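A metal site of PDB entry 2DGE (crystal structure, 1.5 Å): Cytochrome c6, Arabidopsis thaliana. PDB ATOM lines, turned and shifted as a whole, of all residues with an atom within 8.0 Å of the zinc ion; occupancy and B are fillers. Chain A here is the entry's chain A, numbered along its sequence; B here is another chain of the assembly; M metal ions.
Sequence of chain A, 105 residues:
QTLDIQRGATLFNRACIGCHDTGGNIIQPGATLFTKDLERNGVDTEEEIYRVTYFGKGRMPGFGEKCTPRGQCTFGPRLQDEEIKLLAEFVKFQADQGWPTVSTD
The zinc ion is bound by OE2 of Glu 89 of chain B (2.0 Å), OD2 of Asp 4 of chain B (2.0 Å), OD1 of Asp 4 of chain A (2.0 Å) and OE2 of Glu 89 of chain A (2.0 Å). Slightly farther from the zinc ion lies the side-chain carboxylate (OE1) of Glu 89 of chain A (2.8 Å). Slightly farther from the zinc ion lies OE1 of Glu 89 of chain B (2.8 Å).
NZ of Lys 85 of chain B touches the zinc ion, at 3.7 Å. Five residues have an atom within 4 Å of the zinc ion: Asp 4 of chain A, Glu 89 of chain A, Asp 4 of chain B, Lys 85 of chain B and Glu 89 of chain B. The nearest printed residue that does not touch the zinc ion is Leu 86 of chain B (5.2 Å).
OE1 of Glu 89 of chain B is in salt-bridge range of NZ of Lys 85 of chain B (2.8 Å). OD2 of Asp 4 of chain B sits close to NZ of Lys 85 of chain B (3.3 Å). The side-chain carboxylate (OD2) of Asp 4 of chain A lies within salt-bridge range of the side-chain amino group (NZ) of Lys 85 of chain B. OD2 of Asp 4 of chain A is in salt-bridge range of NH1 of Arg 7 (2.9 Å).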
ATOM      1  N   THR A   2      32.061   0.739   2.172  1.00  0.00           N
ATOM      2  CA  THR A   2      30.899   0.847   3.064  1.00  0.00           C
ATOM      3  C   THR A   2      30.812  -0.378   3.952  1.00  0.00           C
ATOM      4  O   THR A   2      31.382  -1.416   3.627  1.00  0.00           O
ATOM      5  CB  THR A   2      29.572   0.974   2.302  1.00  0.00           C
ATOM      6  OG1 THR A   2      29.418  -0.159   1.432  1.00  0.00           O
ATOM      7  CG2 THR A   2      29.552   2.197   1.378  1.00  0.00           C
ATOM      8  N   LEU A   3      30.037  -0.270   5.019  1.00  0.00           N
ATOM      9  CA  LEU A   3      29.811  -1.407   5.903  1.00  0.00           C
ATOM     10  C   LEU A   3      29.147  -2.552   5.161  1.00  0.00           C
ATOM     11  O   LEU A   3      29.563  -3.710   5.317  1.00  0.00           O
ATOM     12  CB  LEU A   3      28.972  -0.993   7.116  1.00  0.00           C
ATOM     13  CG  LEU A   3      29.645   0.036   8.028  1.00  0.00           C
ATOM     14  CD1 LEU A   3      28.629   0.627   8.966  1.00  0.00           C
ATOM     15  CD2 LEU A   3      30.785  -0.616   8.787  1.00  0.00           C
ATOM     16  N   ASP A   4      28.151  -2.239   4.320  1.00  0.00           N
ATOM     17  CA  ASP A   4      27.478  -3.283   3.557  1.00  0.00           C
ATOM     18  C   ASP A   4      28.419  -4.091   2.665  1.00  0.00           C
ATOM     19  O   ASP A   4      28.241  -5.298   2.544  1.00  0.00           O
ATOM     20  CB  ASP A   4      26.308  -2.729   2.746  1.00  0.00           C
ATOM     21  CG  ASP A   4      25.051  -2.629   3.570  1.00  0.00           C
ATOM     22  OD1 ASP A   4      24.021  -2.167   3.043  1.00  0.00           O
ATOM     23  OD2 ASP A   4      25.006  -3.000   4.772  1.00  0.00           O
ATOM     24  N   ILE A   5      29.390  -3.447   2.026  1.00  0.00           N
ATOM     25  CA  ILE A   5      30.315  -4.203   1.179  1.00  0.00           C
ATOM     26  C   ILE A   5      31.239  -5.062   2.048  1.00  0.00           C
ATOM     27  O   ILE A   5      31.565  -6.187   1.674  1.00  0.00           O
ATOM     28  CB  ILE A   5      31.024  -3.301   0.145  1.00  0.00           C
ATOM     29  CG1 ILE A   5      29.980  -2.708  -0.823  1.00  0.00           C
ATOM     30  CG2 ILE A   5      32.106  -4.048  -0.636  1.00  0.00           C
ATOM     31  CD1 ILE A   5      29.112  -3.728  -1.591  1.00  0.00           C
ATOM     32  N   ARG A   7      30.357  -6.418   4.932  1.00  0.00           N
ATOM     33  CA  ARG A   7      29.503  -7.491   5.430  1.00  0.00           C
ATOM     34  C   ARG A   7      29.297  -8.535   4.341  1.00  0.00           C
ATOM     35  O   ARG A   7      29.300  -9.738   4.607  1.00  0.00           O
ATOM     36  CB  ARG A   7      28.152  -6.939   5.847  1.00  0.00           C
ATOM     37  CG  ARG A   7      28.215  -6.023   7.067  1.00  0.00           C
ATOM     38  CD  ARG A   7      27.027  -5.089   7.169  1.00  0.00           C
ATOM     39  NE  ARG A   7      27.045  -4.316   8.405  1.00  0.00           N
ATOM     40  CZ  ARG A   7      26.403  -3.169   8.581  1.00  0.00           C
ATOM     41  NH1 ARG A   7      25.695  -2.619   7.589  1.00  0.00           N
ATOM     42  NH2 ARG A   7      26.461  -2.551   9.754  1.00  0.00           N
ATOM     43  N   GLU A  46      20.135  -7.022  -9.298  1.00  0.00           N
ATOM     44  CA  GLU A  46      20.169  -7.566  -7.936  1.00  0.00           C
ATOM     45  C   GLU A  46      19.033  -8.545  -7.653  1.00  0.00           C
ATOM     46  O   GLU A  46      19.220  -9.523  -6.942  1.00  0.00           O
ATOM     47  CB  GLU A  46      20.143  -6.444  -6.906  1.00  0.00           C
ATOM     48  CG  GLU A  46      21.491  -6.138  -6.325  1.00  0.00           C
ATOM     49  CD  GLU A  46      21.472  -4.846  -5.552  1.00  0.00           C
ATOM     50  OE1 GLU A  46      21.485  -4.905  -4.323  1.00  0.00           O
ATOM     51  OE2 GLU A  46      21.431  -3.783  -6.200  1.00  0.00           O
ATOM     52  N   GLU A  82      18.331 -11.815   4.678  1.00  0.00           N
ATOM     53  CA  GLU A  82      19.169 -10.617   4.748  1.00  0.00           C
ATOM     54  C   GLU A  82      20.602 -10.888   4.278  1.00  0.00           C
ATOM     55  O   GLU A  82      21.267 -10.001   3.731  1.00  0.00           O
ATOM     56  CB  GLU A  82      19.194 -10.001   6.155  1.00  0.00           C
ATOM     57  CG  GLU A  82      19.137  -8.472   6.180  1.00  0.00           C
ATOM     58  CD  GLU A  82      20.466  -7.806   5.848  1.00  0.00           C
ATOM     59  OE1 GLU A  82      20.668  -7.434   4.674  1.00  0.00           O
ATOM     60  OE2 GLU A  82      21.308  -7.636   6.776  1.00  0.00           O
ATOM     61  N   LYS A  85      20.434 -11.032   0.520  1.00  0.00           N
ATOM     62  CA  LYS A  85      20.326  -9.631   0.123  1.00  0.00           C
ATOM     63  C   LYS A  85      21.689  -8.932   0.094  1.00  0.00           C
ATOM     64  O   LYS A  85      22.016  -8.232  -0.872  1.00  0.00           O
ATOM     65  CB  LYS A  85      19.391  -8.900   1.105  1.00  0.00           C
ATOM     66  CG  LYS A  85      18.872  -7.554   0.643  1.00  0.00           C
ATOM     67  CD  LYS A  85      17.551  -7.226   1.371  1.00  0.00           C
ATOM     68  CE  LYS A  85      16.412  -6.920   0.413  1.00  0.00           C
ATOM     69  NZ  LYS A  85      15.790  -8.144  -0.180  1.00  0.00           N
ATOM     70  N   LEU A  86      22.489  -9.118   1.152  1.00  0.00           N
ATOM     71  CA  LEU A  86      23.830  -8.570   1.212  1.00  0.00           C
ATOM     72  C   LEU A  86      24.721  -9.146   0.114  1.00  0.00           C
ATOM     73  O   LEU A  86      25.516  -8.434  -0.476  1.00  0.00           O
ATOM     74  CB  LEU A  86      24.489  -8.868   2.570  1.00  0.00           C
ATOM     75  CG  LEU A  86      24.888  -7.818   3.618  1.00  0.00           C
ATOM     76  CD1 LEU A  86      24.571  -6.360   3.273  1.00  0.00           C
ATOM     77  CD2 LEU A  86      24.382  -8.176   4.980  1.00  0.00           C
ATOM     78  N   GLU A  89      23.857  -7.622  -3.280  1.00  0.00           N
ATOM     79  CA  GLU A  89      24.443  -6.280  -3.285  1.00  0.00           C
ATOM     80  C   GLU A  89      25.933  -6.341  -3.546  1.00  0.00           C
ATOM     81  O   GLU A  89      26.455  -5.560  -4.340  1.00  0.00           O
ATOM     82  CB  GLU A  89      24.139  -5.598  -1.944  1.00  0.00           C
ATOM     83  CG  GLU A  89      24.711  -4.191  -1.830  1.00  0.00           C
ATOM     84  CD  GLU A  89      24.393  -3.523  -0.511  1.00  0.00           C
ATOM     85  OE1 GLU A  89      23.794  -4.177   0.376  1.00  0.00           O
ATOM     86  OE2 GLU A  89      24.736  -2.344  -0.389  1.00  0.00           O
ATOM     87  N   PHE A  90      26.600  -7.289  -2.884  1.00  0.00           N
ATOM     88  CA  PHE A  90      28.045  -7.479  -3.012  1.00  0.00           C
ATOM     89  C   PHE A  90      28.415  -7.815  -4.451  1.00  0.00           C
ATOM     90  O   PHE A  90      29.286  -7.174  -5.032  1.00  0.00           O
ATOM     91  CB  PHE A  90      28.543  -8.579  -2.045  1.00  0.00           C
ATOM     92  CG  PHE A  90      30.037  -8.764  -2.086  1.00  0.00           C
ATOM     93  CD1 PHE A  90      30.882  -7.824  -1.498  1.00  0.00           C
ATOM     94  CD2 PHE A  90      30.606  -9.884  -2.702  1.00  0.00           C
ATOM     95  CE1 PHE A  90      32.282  -7.987  -1.530  1.00  0.00           C
ATOM     96  CE2 PHE A  90      31.982 -10.065  -2.733  1.00  0.00           C
ATOM     97  CZ  PHE A  90      32.840  -9.126  -2.140  1.00  0.00           C
ATOM     98  N   THR B   2      23.747  -0.096  -7.212  1.00  0.00           N
ATOM     99  CA  THR B   2      22.968  -1.033  -6.425  1.00  0.00           C
ATOM    100  C   THR B   2      21.665  -0.394  -6.002  1.00  0.00           C
ATOM    101  O   THR B   2      21.507   0.839  -6.069  1.00  0.00           O
ATOM    102  CB  THR B   2      23.738  -1.456  -5.172  1.00  0.00           C
ATOM    103  OG1 THR B   2      24.009  -0.289  -4.378  1.00  0.00           O
ATOM    104  CG2 THR B   2      25.126  -2.011  -5.530  1.00  0.00           C
ATOM    105  N   LEU B   3      20.737  -1.224  -5.533  1.00  0.00           N
ATOM    106  CA  LEU B   3      19.481  -0.734  -5.000  1.00  0.00           C
ATOM    107  C   LEU B   3      19.703   0.192  -3.815  1.00  0.00           C
ATOM    108  O   LEU B   3      19.046   1.231  -3.709  1.00  0.00           O
ATOM    109  CB  LEU B   3      18.539  -1.896  -4.618  1.00  0.00           C
ATOM    110  CG  LEU B   3      18.146  -2.851  -5.761  1.00  0.00           C
ATOM    111  CD1 LEU B   3      17.589  -4.151  -5.178  1.00  0.00           C
ATOM    112  CD2 LEU B   3      17.158  -2.203  -6.708  1.00  0.00           C
ATOM    113  N   ASP B   4      20.655  -0.143  -2.943  1.00  0.00           N
ATOM    114  CA  ASP B   4      20.901   0.715  -1.771  1.00  0.00           C
ATOM    115  C   ASP B   4      21.385   2.101  -2.180  1.00  0.00           C
ATOM    116  O   ASP B   4      20.967   3.109  -1.593  1.00  0.00           O
ATOM    117  CB  ASP B   4      21.886   0.086  -0.792  1.00  0.00           C
ATOM    118  CG  ASP B   4      21.227  -0.907   0.143  1.00  0.00           C
ATOM    119  OD1 ASP B   4      20.003  -1.172   0.019  1.00  0.00           O
ATOM    120  OD2 ASP B   4      21.890  -1.482   1.016  1.00  0.00           O
ATOM    121  N   ILE B   5      22.270   2.165  -3.175  1.00  0.00           N
ATOM    122  CA  ILE B   5      22.753   3.458  -3.633  1.00  0.00           C
ATOM    123  C   ILE B   5      21.640   4.252  -4.326  1.00  0.00           C
ATOM    124  O   ILE B   5      21.470   5.446  -4.065  1.00  0.00           O
ATOM    125  CB  ILE B   5      24.009   3.318  -4.499  1.00  0.00           C
ATOM    126  CG1 ILE B   5      25.206   2.872  -3.626  1.00  0.00           C
ATOM    127  CG2 ILE B   5      24.303   4.625  -5.225  1.00  0.00           C
ATOM    128  CD1 ILE B   5      25.472   3.765  -2.366  1.00  0.00           C
ATOM    129  N   GLU B  46      31.384   5.609   8.670  1.00  0.00           N
ATOM    130  CA  GLU B  46      29.992   5.523   8.306  1.00  0.00           C
ATOM    131  C   GLU B  46      29.082   5.623   9.557  1.00  0.00           C
ATOM    132  O   GLU B  46      28.001   6.204   9.515  1.00  0.00           O
ATOM    133  CB  GLU B  46      29.768   4.209   7.564  1.00  0.00           C
ATOM    134  CG  GLU B  46      28.559   4.207   6.682  1.00  0.00           C
ATOM    135  CD  GLU B  46      28.455   2.951   5.860  1.00  0.00           C
ATOM    136  OE1 GLU B  46      27.313   2.496   5.640  1.00  0.00           O
ATOM    137  OE2 GLU B  46      29.521   2.406   5.469  1.00  0.00           O
ATOM    138  N   GLU B  82      16.191   3.271   8.980  1.00  0.00           N
ATOM    139  CA  GLU B  82      16.672   2.606   7.769  1.00  0.00           C
ATOM    140  C   GLU B  82      17.028   3.635   6.701  1.00  0.00           C
ATOM    141  O   GLU B  82      17.978   3.444   5.943  1.00  0.00           O
ATOM    142  CB  GLU B  82      15.625   1.614   7.260  1.00  0.00           C
ATOM    143  CG  GLU B  82      15.992   0.965   5.937  1.00  0.00           C
ATOM    144  CD  GLU B  82      17.108  -0.050   6.079  1.00  0.00           C
ATOM    145  OE1 GLU B  82      17.483  -0.383   7.227  1.00  0.00           O
ATOM    146  OE2 GLU B  82      17.620  -0.510   5.028  1.00  0.00           O
ATOM    147  N   LYS B  85      20.323   5.093   7.737  1.00  0.00           N
ATOM    148  CA  LYS B  85      21.334   4.101   7.422  1.00  0.00           C
ATOM    149  C   LYS B  85      21.717   4.179   5.930  1.00  0.00           C
ATOM    150  O   LYS B  85      22.893   4.176   5.585  1.00  0.00           O
ATOM    151  CB  LYS B  85      20.824   2.701   7.761  1.00  0.00           C
ATOM    152  CG  LYS B  85      21.755   1.560   7.379  1.00  0.00           C
ATOM    153  CD  LYS B  85      21.336   0.923   6.038  1.00  0.00           C
ATOM    154  CE  LYS B  85      22.293  -0.174   5.637  1.00  0.00           C
ATOM    155  NZ  LYS B  85      22.031  -0.616   4.236  1.00  0.00           N
ATOM    156  N   LEU B  86      20.702   4.239   5.065  1.00  0.00           N
ATOM    157  CA  LEU B  86      20.943   4.346   3.626  1.00  0.00           C
ATOM    158  C   LEU B  86      21.647   5.646   3.246  1.00  0.00           C
ATOM    159  O   LEU B  86      22.485   5.660   2.359  1.00  0.00           O
ATOM    160  CB  LEU B  86      19.647   4.184   2.841  1.00  0.00           C
ATOM    161  CG  LEU B  86      19.094   2.751   2.829  1.00  0.00           C
ATOM    162  CD1 LEU B  86      17.695   2.755   2.284  1.00  0.00           C
ATOM    163  CD2 LEU B  86      20.001   1.871   1.953  1.00  0.00           C
ATOM    164  N   GLU B  89      25.314   5.357   4.240  1.00  0.00           N
ATOM    165  CA  GLU B  89      25.907   4.494   3.238  1.00  0.00           C
ATOM    166  C   GLU B  89      26.171   5.267   1.946  1.00  0.00           C
ATOM    167  O   GLU B  89      27.255   5.158   1.360  1.00  0.00           O
ATOM    168  CB  GLU B  89      24.970   3.302   2.996  1.00  0.00           C
ATOM    169  CG  GLU B  89      25.429   2.336   1.933  1.00  0.00           C
ATOM    170  CD  GLU B  89      24.538   1.117   1.803  1.00  0.00           C
ATOM    171  OE1 GLU B  89      23.474   1.056   2.448  1.00  0.00           O
ATOM    172  OE2 GLU B  89      24.901   0.215   1.044  1.00  0.00           O
ATOM    173  N   PHE B  90      25.191   6.069   1.531  1.00  0.00           N
ATOM    174  CA  PHE B  90      25.295   6.890   0.318  1.00  0.00           C
ATOM    175  C   PHE B  90      26.430   7.906   0.443  1.00  0.00           C
ATOM    176  O   PHE B  90      27.239   8.043  -0.451  1.00  0.00           O
ATOM    177  CB  PHE B  90      23.974   7.606   0.019  1.00  0.00           C
ATOM    178  CG  PHE B  90      23.994   8.377  -1.254  1.00  0.00           C
ATOM    179  CD1 PHE B  90      23.990   7.731  -2.489  1.00  0.00           C
ATOM    180  CD2 PHE B  90      24.014   9.766  -1.231  1.00  0.00           C
ATOM    181  CE1 PHE B  90      24.016   8.469  -3.688  1.00  0.00           C
ATOM    182  CE2 PHE B  90      24.026  10.513  -2.412  1.00  0.00           C
ATOM    183  CZ  PHE B  90      24.040   9.872  -3.634  1.00  0.00           C
HETATM  184 ZN    ZN M   1      23.862  -1.455   1.182  1.00  0.00          ZN
